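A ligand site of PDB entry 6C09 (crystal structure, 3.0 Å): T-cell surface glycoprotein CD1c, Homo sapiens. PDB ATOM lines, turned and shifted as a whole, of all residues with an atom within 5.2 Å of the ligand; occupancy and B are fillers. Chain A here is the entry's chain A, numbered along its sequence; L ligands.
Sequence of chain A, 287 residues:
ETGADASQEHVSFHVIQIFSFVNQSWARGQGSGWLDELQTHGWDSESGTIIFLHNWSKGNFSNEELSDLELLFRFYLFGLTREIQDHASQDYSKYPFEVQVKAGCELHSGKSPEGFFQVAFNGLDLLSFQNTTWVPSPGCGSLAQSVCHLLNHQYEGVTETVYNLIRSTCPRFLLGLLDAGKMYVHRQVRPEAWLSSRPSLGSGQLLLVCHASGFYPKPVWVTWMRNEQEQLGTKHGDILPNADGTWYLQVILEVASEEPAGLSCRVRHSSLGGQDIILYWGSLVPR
An oxygen (O3) of the ligand lies close to the backbone carbonyl oxygen of Gly 29, 3.1 Å away. The backbone NH (N) of Gln 30 sits at hydrogen-bond distance from an oxygen (O3) of the ligand, 3.1 Å away. The side-chain amide nitrogen (NE2) of Gln 17 sits close to an oxygen (O2) of the ligand, at 3.4 Å. O3 of the ligand lies within hydrogen-bond range of N of Gly 31 (3.4 Å).
OG of Ser 45 lies within hydrogen-bond range of O of Gly 29 (3.1 Å). The backbone carbonyl oxygen of Gly 31 lies within hydrogen-bond range of the backbone NH of Trp 43, 3.5 Å away. The backbone NH of Ile 18 lies within hydrogen-bond range of the backbone carbonyl oxygen of Gln 30 (2.9 Å). The backbone NH (N) of Gly 33 lies within hydrogen-bond range of the backbone carbonyl oxygen (O) of His 41. The backbone carbonyl oxygen (O) of Ser 32 lies within hydrogen-bond range of the backbone NH (N) of Ile 16 (2.9 Å). The backbone carbonyl oxygen (O) of Ala 103 is in hydrogen-bond range of the backbone NH (N) of Val 15 (2.8 Å). N of Cys 170 lies within hydrogen-bond range of O of Leu 165 (2.8 Å).
Merely in contact with the ligand: Trp 43 (3.1 Å), His 41 (3.4 Å), Leu 77 (3.6 Å), Phe 173 (3.6 Å), Phe 19 (3.7 Å), Ser 45 (3.7 Å), Phe 13 (3.8 Å), Ser 32 (3.8 Å), Val 15 (3.8 Å), Leu 69 (3.8 Å), Ile 50 (3.9 Å), Cys 170 (3.9 Å), Phe 73 (3.96 Å), Gly 33 (3.99 Å), Leu 165 (3.99 Å) and Ile 16 (3.99 Å). Hydrophobic or aromatic side chains within 4 Å of the ligand: Phe 13, Val 15, Phe 19, His 41, Trp 43, Ile 50, Leu 69, Phe 73, Leu 77, Leu 165 and Phe 173. 20 residues have an atom within 4 Å of the ligand: Phe 13, Val 15, Ile 16, Gln 17, Phe 19, Gly 29, Gln 30, Gly 31, Ser 32, Gly 33, His 41, Trp 43, Ser 45, Ile 50, Leu 69, Phe 73, Leu 77, Leu 165, Cys 170 and Phe 173. The nearest printed residue that does not touch the ligand is Ala 103 (4.1 Å).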
ATOM      1  N   PHE A  13      22.809  19.359 -16.284  1.00  0.00           N
ATOM      2  CA  PHE A  13      22.751  20.329 -15.184  1.00  0.00           C
ATOM      3  C   PHE A  13      21.539  19.979 -14.290  1.00  0.00           C
ATOM      4  O   PHE A  13      20.519  19.498 -14.793  1.00  0.00           O
ATOM      5  CB  PHE A  13      22.675  21.765 -15.668  1.00  0.00           C
ATOM      6  CG  PHE A  13      22.806  22.750 -14.532  1.00  0.00           C
ATOM      7  CD1 PHE A  13      24.042  22.998 -13.943  1.00  0.00           C
ATOM      8  CD2 PHE A  13      21.702  23.434 -14.056  1.00  0.00           C
ATOM      9  CE1 PHE A  13      24.158  23.897 -12.880  1.00  0.00           C
ATOM     10  CE2 PHE A  13      21.826  24.335 -12.998  1.00  0.00           C
ATOM     11  CZ  PHE A  13      23.053  24.562 -12.415  1.00  0.00           C
ATOM     12  N   VAL A  15      19.764  21.073 -10.055  1.00  0.00           N
ATOM     13  CA  VAL A  15      19.803  21.730  -8.762  1.00  0.00           C
ATOM     14  C   VAL A  15      19.223  20.738  -7.762  1.00  0.00           C
ATOM     15  O   VAL A  15      18.456  19.851  -8.135  1.00  0.00           O
ATOM     16  CB  VAL A  15      19.134  23.134  -8.690  1.00  0.00           C
ATOM     17  CG1 VAL A  15      19.453  23.959  -9.938  1.00  0.00           C
ATOM     18  CG2 VAL A  15      17.638  23.061  -8.491  1.00  0.00           C
ATOM     19  N   ILE A  16      19.671  20.820  -6.526  1.00  0.00           N
ATOM     20  CA  ILE A  16      19.164  19.941  -5.484  1.00  0.00           C
ATOM     21  C   ILE A  16      18.645  20.820  -4.353  1.00  0.00           C
ATOM     22  O   ILE A  16      19.239  21.852  -4.033  1.00  0.00           O
ATOM     23  CB  ILE A  16      20.164  18.824  -5.003  1.00  0.00           C
ATOM     24  CG1 ILE A  16      21.380  19.410  -4.273  1.00  0.00           C
ATOM     25  CG2 ILE A  16      20.579  17.873  -6.146  1.00  0.00           C
ATOM     26  CD1 ILE A  16      22.014  18.515  -3.309  1.00  0.00           C
ATOM     27  N   GLN A  17      17.510  20.434  -3.773  1.00  0.00           N
ATOM     28  CA  GLN A  17      16.955  21.183  -2.648  1.00  0.00           C
ATOM     29  C   GLN A  17      16.679  20.212  -1.549  1.00  0.00           C
ATOM     30  O   GLN A  17      16.074  19.191  -1.818  1.00  0.00           O
ATOM     31  CB  GLN A  17      15.676  21.942  -3.052  1.00  0.00           C
ATOM     32  CG  GLN A  17      15.886  22.830  -4.253  1.00  0.00           C
ATOM     33  CD  GLN A  17      14.620  23.274  -4.907  1.00  0.00           C
ATOM     34  OE1 GLN A  17      13.621  22.553  -4.949  1.00  0.00           O
ATOM     35  NE2 GLN A  17      14.663  24.451  -5.504  1.00  0.00           N
ATOM     36  N   ILE A  18      17.197  20.477  -0.348  1.00  0.00           N
ATOM     37  CA  ILE A  18      16.993  19.623   0.838  1.00  0.00           C
ATOM     38  C   ILE A  18      16.179  20.421   1.876  1.00  0.00           C
ATOM     39  O   ILE A  18      16.713  21.364   2.476  1.00  0.00           O
ATOM     40  CB  ILE A  18      18.328  19.019   1.408  1.00  0.00           C
ATOM     41  N   PHE A  19      14.862  20.107   1.998  1.00  0.00           N
ATOM     42  CA  PHE A  19      13.927  20.758   2.929  1.00  0.00           C
ATOM     43  C   PHE A  19      13.727  19.931   4.159  1.00  0.00           C
ATOM     44  O   PHE A  19      13.299  18.781   4.066  1.00  0.00           O
ATOM     45  CB  PHE A  19      12.562  21.004   2.291  1.00  0.00           C
ATOM     46  CG  PHE A  19      12.632  21.838   1.040  1.00  0.00           C
ATOM     47  CD1 PHE A  19      12.910  23.196   1.114  1.00  0.00           C
ATOM     48  CD2 PHE A  19      12.467  21.262  -0.208  1.00  0.00           C
ATOM     49  CE1 PHE A  19      13.040  23.948  -0.046  1.00  0.00           C
ATOM     50  CE2 PHE A  19      12.589  22.011  -1.363  1.00  0.00           C
ATOM     51  CZ  PHE A  19      12.889  23.352  -1.278  1.00  0.00           C
ATOM     52  N   ARG A  28      13.858  24.333   7.418  1.00  0.00           N
ATOM     53  CA  ARG A  28      15.090  24.840   6.777  1.00  0.00           C
ATOM     54  C   ARG A  28      15.388  24.234   5.395  1.00  0.00           C
ATOM     55  O   ARG A  28      15.125  23.068   5.144  1.00  0.00           O
ATOM     56  CB  ARG A  28      16.321  24.704   7.703  1.00  0.00           C
ATOM     57  CG  ARG A  28      16.226  25.495   9.014  1.00  0.00           C
ATOM     58  CD  ARG A  28      15.970  27.010   8.911  1.00  0.00           C
ATOM     59  NE  ARG A  28      14.642  27.373   9.435  1.00  0.00           N
ATOM     60  CZ  ARG A  28      14.174  28.611   9.534  1.00  0.00           C
ATOM     61  NH1 ARG A  28      12.952  28.838  10.010  1.00  0.00           N
ATOM     62  NH2 ARG A  28      14.931  29.650   9.177  1.00  0.00           N
ATOM     63  N   GLY A  29      15.927  25.058   4.516  1.00  0.00           N
ATOM     64  CA  GLY A  29      16.279  24.646   3.164  1.00  0.00           C
ATOM     65  C   GLY A  29      17.743  24.835   2.813  1.00  0.00           C
ATOM     66  O   GLY A  29      18.405  25.771   3.277  1.00  0.00           O
ATOM     67  N   GLN A  30      18.254  23.926   1.982  1.00  0.00           N
ATOM     68  CA  GLN A  30      19.629  23.926   1.517  1.00  0.00           C
ATOM     69  C   GLN A  30      19.524  23.742   0.039  1.00  0.00           C
ATOM     70  O   GLN A  30      18.646  23.007  -0.419  1.00  0.00           O
ATOM     71  CB  GLN A  30      20.403  22.737   2.107  1.00  0.00           C
ATOM     72  CG  GLN A  30      20.808  22.907   3.549  1.00  0.00           C
ATOM     73  CD  GLN A  30      22.009  22.078   3.881  1.00  0.00           C
ATOM     74  OE1 GLN A  30      23.091  22.220   3.269  1.00  0.00           O
ATOM     75  NE2 GLN A  30      21.875  21.250   4.905  1.00  0.00           N
ATOM     76  N   GLY A  31      20.405  24.387  -0.730  1.00  0.00           N
ATOM     77  CA  GLY A  31      20.374  24.246  -2.179  1.00  0.00           C
ATOM     78  C   GLY A  31      21.714  24.350  -2.873  1.00  0.00           C
ATOM     79  O   GLY A  31      22.644  24.974  -2.353  1.00  0.00           O
ATOM     80  N   SER A  32      21.802  23.727  -4.064  1.00  0.00           N
ATOM     81  CA  SER A  32      23.035  23.748  -4.849  1.00  0.00           C
ATOM     82  C   SER A  32      22.816  23.456  -6.313  1.00  0.00           C
ATOM     83  O   SER A  32      21.851  22.771  -6.668  1.00  0.00           O
ATOM     84  CB  SER A  32      24.108  22.809  -4.269  1.00  0.00           C
ATOM     85  OG  SER A  32      23.627  21.605  -3.699  1.00  0.00           O
ATOM     86  N   GLY A  33      23.751  23.952  -7.125  1.00  0.00           N
ATOM     87  CA  GLY A  33      23.831  23.762  -8.566  1.00  0.00           C
ATOM     88  C   GLY A  33      24.939  22.770  -8.890  1.00  0.00           C
ATOM     89  O   GLY A  33      26.016  22.862  -8.308  1.00  0.00           O
ATOM     90  N   HIS A  41      27.294  25.888  -8.111  1.00  0.00           N
ATOM     91  CA  HIS A  41      26.552  26.907  -7.392  1.00  0.00           C
ATOM     92  C   HIS A  41      26.163  26.504  -6.010  1.00  0.00           C
ATOM     93  O   HIS A  41      25.858  25.335  -5.749  1.00  0.00           O
ATOM     94  CB  HIS A  41      25.249  27.218  -8.120  1.00  0.00           C
ATOM     95  CG  HIS A  41      25.426  27.582  -9.548  1.00  0.00           C
ATOM     96  ND1 HIS A  41      25.319  26.625 -10.537  1.00  0.00           N
ATOM     97  CD2 HIS A  41      25.704  28.773 -10.111  1.00  0.00           C
ATOM     98  CE1 HIS A  41      25.541  27.269 -11.668  1.00  0.00           C
ATOM     99  NE2 HIS A  41      25.765  28.567 -11.463  1.00  0.00           N
ATOM    100  N   GLY A  42      26.039  27.504  -5.169  1.00  0.00           N
ATOM    101  CA  GLY A  42      25.511  27.345  -3.833  1.00  0.00           C
ATOM    102  C   GLY A  42      24.276  28.211  -3.704  1.00  0.00           C
ATOM    103  O   GLY A  42      23.831  28.818  -4.682  1.00  0.00           O
ATOM    104  N   TRP A  43      23.706  28.265  -2.489  1.00  0.00           N
ATOM    105  CA  TRP A  43      22.530  29.098  -2.245  1.00  0.00           C
ATOM    106  C   TRP A  43      22.632  29.695  -0.861  1.00  0.00           C
ATOM    107  O   TRP A  43      22.723  28.950   0.124  1.00  0.00           O
ATOM    108  CB  TRP A  43      21.222  28.291  -2.451  1.00  0.00           C
ATOM    109  CG  TRP A  43      19.945  29.062  -2.210  1.00  0.00           C
ATOM    110  CD1 TRP A  43      19.167  29.031  -1.079  1.00  0.00           C
ATOM    111  CD2 TRP A  43      19.271  29.933  -3.130  1.00  0.00           C
ATOM    112  NE1 TRP A  43      18.065  29.838  -1.237  1.00  0.00           N
ATOM    113  CE2 TRP A  43      18.104  30.407  -2.487  1.00  0.00           C
ATOM    114  CE3 TRP A  43      19.513  30.339  -4.457  1.00  0.00           C
ATOM    115  CZ2 TRP A  43      17.202  31.275  -3.114  1.00  0.00           C
ATOM    116  CZ3 TRP A  43      18.635  31.220  -5.074  1.00  0.00           C
ATOM    117  CH2 TRP A  43      17.498  31.687  -4.402  1.00  0.00           C
ATOM    118  N   SER A  45      20.747  30.930   1.835  1.00  0.00           N
ATOM    119  CA  SER A  45      19.360  30.817   2.281  1.00  0.00           C
ATOM    120  C   SER A  45      18.863  32.094   2.917  1.00  0.00           C
ATOM    121  O   SER A  45      17.689  32.421   2.768  1.00  0.00           O
ATOM    122  CB  SER A  45      19.199  29.659   3.259  1.00  0.00           C
ATOM    123  OG  SER A  45      19.858  28.489   2.787  1.00  0.00           O
ATOM    124  N   ILE A  50      22.064  33.147  -5.205  1.00  0.00           N
ATOM    125  CA  ILE A  50      22.940  32.096  -5.690  1.00  0.00           C
ATOM    126  C   ILE A  50      24.353  32.428  -5.228  1.00  0.00           C
ATOM    127  O   ILE A  50      24.698  33.605  -5.079  1.00  0.00           O
ATOM    128  CB  ILE A  50      22.872  31.992  -7.254  1.00  0.00           C
ATOM    129  CG1 ILE A  50      21.442  31.651  -7.752  1.00  0.00           C
ATOM    130  CG2 ILE A  50      23.915  30.987  -7.816  1.00  0.00           C
ATOM    131  CD1 ILE A  50      21.170  32.040  -9.156  1.00  0.00           C
ATOM    132  N   LEU A  69      16.295  34.741 -11.770  1.00  0.00           N
ATOM    133  CA  LEU A  69      16.264  33.322 -11.433  1.00  0.00           C
ATOM    134  C   LEU A  69      16.152  33.219  -9.922  1.00  0.00           C
ATOM    135  O   LEU A  69      15.346  32.440  -9.433  1.00  0.00           O
ATOM    136  CB  LEU A  69      17.506  32.593 -11.893  1.00  0.00           C
ATOM    137  CG  LEU A  69      17.402  31.983 -13.264  1.00  0.00           C
ATOM    138  CD1 LEU A  69      18.781  31.822 -13.915  1.00  0.00           C
ATOM    139  CD2 LEU A  69      16.652  30.655 -13.222  1.00  0.00           C
ATOM    140  N   PHE A  73      13.294  31.512  -7.813  1.00  0.00           N
ATOM    141  CA  PHE A  73      13.593  30.524  -6.762  1.00  0.00           C
ATOM    142  C   PHE A  73      12.991  30.883  -5.401  1.00  0.00           C
ATOM    143  O   PHE A  73      12.364  30.024  -4.794  1.00  0.00           O
ATOM    144  CB  PHE A  73      15.086  30.264  -6.612  1.00  0.00           C
ATOM    145  CG  PHE A  73      15.687  29.496  -7.751  1.00  0.00           C
ATOM    146  CD1 PHE A  73      15.154  28.280  -8.141  1.00  0.00           C
ATOM    147  CD2 PHE A  73      16.836  29.943  -8.383  1.00  0.00           C
ATOM    148  CE1 PHE A  73      15.703  27.565  -9.217  1.00  0.00           C
ATOM    149  CE2 PHE A  73      17.407  29.208  -9.426  1.00  0.00           C
ATOM    150  CZ  PHE A  73      16.835  28.026  -9.828  1.00  0.00           C
ATOM    151  N   LEU A  77      10.153  28.897  -3.182  1.00  0.00           N
ATOM    152  CA  LEU A  77      10.414  28.537  -1.784  1.00  0.00           C
ATOM    153  C   LEU A  77       9.315  29.092  -0.927  1.00  0.00           C
ATOM    154  O   LEU A  77       8.750  28.345  -0.124  1.00  0.00           O
ATOM    155  CB  LEU A  77      11.784  29.006  -1.332  1.00  0.00           C
ATOM    156  CG  LEU A  77      12.945  28.417  -2.133  1.00  0.00           C
ATOM    157  CD1 LEU A  77      14.263  29.040  -1.763  1.00  0.00           C
ATOM    158  CD2 LEU A  77      12.962  26.881  -2.096  1.00  0.00           C
ATOM    159  N   ALA A 103      16.029  18.709  -9.744  1.00  0.00           N
ATOM    160  CA  ALA A 103      15.442  19.193 -10.965  1.00  0.00           C
ATOM    161  C   ALA A 103      16.515  19.721 -11.873  1.00  0.00           C
ATOM    162  O   ALA A 103      17.448  20.351 -11.389  1.00  0.00           O
ATOM    163  CB  ALA A 103      14.473  20.307 -10.646  1.00  0.00           C
ATOM    164  N   GLY A 104      16.381  19.468 -13.178  1.00  0.00           N
ATOM    165  CA  GLY A 104      17.363  19.906 -14.174  1.00  0.00           C
ATOM    166  C   GLY A 104      17.098  19.444 -15.594  1.00  0.00           C
ATOM    167  O   GLY A 104      15.960  19.137 -15.964  1.00  0.00           O
ATOM    168  N   LEU A 165      11.166  26.048 -17.291  1.00  0.00           N
ATOM    169  CA  LEU A 165      12.422  26.149 -16.566  1.00  0.00           C
ATOM    170  C   LEU A 165      13.339  25.019 -16.927  1.00  0.00           C
ATOM    171  O   LEU A 165      14.457  25.259 -17.352  1.00  0.00           O
ATOM    172  CB  LEU A 165      12.112  26.138 -15.050  1.00  0.00           C
ATOM    173  CG  LEU A 165      13.177  26.461 -14.040  1.00  0.00           C
ATOM    174  CD1 LEU A 165      13.974  27.671 -14.450  1.00  0.00           C
ATOM    175  CD2 LEU A 165      12.525  26.733 -12.733  1.00  0.00           C
ATOM    176  N   ILE A 166      12.849  23.770 -16.750  1.00  0.00           N
ATOM    177  CA  ILE A 166      13.638  22.562 -16.952  1.00  0.00           C
ATOM    178  C   ILE A 166      13.877  22.266 -18.434  1.00  0.00           C
ATOM    179  O   ILE A 166      14.938  21.751 -18.772  1.00  0.00           O
ATOM    180  CB  ILE A 166      13.060  21.359 -16.148  1.00  0.00           C
ATOM    181  CG1 ILE A 166      11.728  20.833 -16.735  1.00  0.00           C
ATOM    182  CG2 ILE A 166      12.929  21.708 -14.655  1.00  0.00           C
ATOM    183  CD1 ILE A 166      11.134  19.612 -16.060  1.00  0.00           C
ATOM    184  N   THR A 169      14.929  27.180 -20.085  1.00  0.00           N
ATOM    185  CA  THR A 169      15.920  27.942 -19.335  1.00  0.00           C
ATOM    186  C   THR A 169      17.136  27.128 -19.011  1.00  0.00           C
ATOM    187  O   THR A 169      18.240  27.618 -19.244  1.00  0.00           O
ATOM    188  CB  THR A 169      15.311  28.584 -18.103  1.00  0.00           C
ATOM    189  OG1 THR A 169      14.214  29.412 -18.502  1.00  0.00           O
ATOM    190  CG2 THR A 169      16.329  29.397 -17.298  1.00  0.00           C
ATOM    191  N   CYS A 170      16.937  25.907 -18.491  1.00  0.00           N
ATOM    192  CA  CYS A 170      18.004  24.982 -18.111  1.00  0.00           C
ATOM    193  C   CYS A 170      18.978  24.689 -19.284  1.00  0.00           C
ATOM    194  O   CYS A 170      20.159  25.041 -19.117  1.00  0.00           O
ATOM    195  CB  CYS A 170      17.442  23.713 -17.487  1.00  0.00           C
ATOM    196  SG  CYS A 170      18.697  22.611 -16.780  1.00  0.00           S
ATOM    197  N   PHE A 173      20.937  27.821 -20.164  1.00  0.00           N
ATOM    198  CA  PHE A 173      21.905  28.045 -19.103  1.00  0.00           C
ATOM    199  C   PHE A 173      23.113  27.115 -19.253  1.00  0.00           C
ATOM    200  O   PHE A 173      24.209  27.612 -19.561  1.00  0.00           O
ATOM    201  CB  PHE A 173      21.279  27.921 -17.714  1.00  0.00           C
ATOM    202  CG  PHE A 173      22.301  28.240 -16.657  1.00  0.00           C
ATOM    203  CD1 PHE A 173      22.870  29.502 -16.570  1.00  0.00           C
ATOM    204  CD2 PHE A 173      22.713  27.264 -15.758  1.00  0.00           C
ATOM    205  CE1 PHE A 173      23.842  29.790 -15.600  1.00  0.00           C
ATOM    206  CE2 PHE A 173      23.700  27.548 -14.807  1.00  0.00           C
ATOM    207  CZ  PHE A 173      24.251  28.808 -14.733  1.00  0.00           C
HETATM  208  C1  LIG L   1      16.128  24.109 -12.512  1.00  0.00           C
HETATM  209  C2  LIG L   1      21.170  27.320 -10.187  1.00  0.00           C
HETATM  210  C3  LIG L   1      21.984  27.317  -8.899  1.00  0.00           C
HETATM  211  C4  LIG L   1      17.418  24.379 -13.301  1.00  0.00           C
HETATM  212  C5  LIG L   1      21.447  28.515 -11.101  1.00  0.00           C
HETATM  213  C6  LIG L   1      21.175  27.720  -7.665  1.00  0.00           C
HETATM  214  C7  LIG L   1      16.603  25.299  -1.346  1.00  0.00           C
HETATM  215  C8  LIG L   1      17.419  25.694 -14.077  1.00  0.00           C
HETATM  216  C9  LIG L   1      21.006  28.256 -12.548  1.00  0.00           C
HETATM  217  C10 LIG L   1      20.691  26.500  -6.890  1.00  0.00           C
HETATM  218  C11 LIG L   1      18.848  26.184 -14.337  1.00  0.00           C
HETATM  219  C12 LIG L   1      19.491  28.118 -12.770  1.00  0.00           C
HETATM  220  C13 LIG L   1      19.800  26.894  -5.726  1.00  0.00           C
HETATM  221  C14 LIG L   1      19.078  27.686 -14.189  1.00  0.00           C
HETATM  222  C15 LIG L   1      18.380  26.379  -5.903  1.00  0.00           C
HETATM  223  C16 LIG L   1      17.973  25.581  -4.675  1.00  0.00           C
HETATM  224  C17 LIG L   1      15.539  26.552   0.558  1.00  0.00           C
HETATM  225  C18 LIG L   1      16.678  26.529  -0.449  1.00  0.00           C
HETATM  226  O1  LIG L   1      17.037  27.547  -3.714  1.00  0.00           O
HETATM  227  C19 LIG L   1      17.096  26.328  -3.672  1.00  0.00           C
HETATM  228  O2  LIG L   1      16.247  25.633  -2.694  1.00  0.00           O
HETATM  229  O3  LIG L   1      17.917  26.534   0.282  1.00  0.00           O
HETATM  230  O4  LIG L   1      15.786  27.522   1.597  1.00  0.00           O
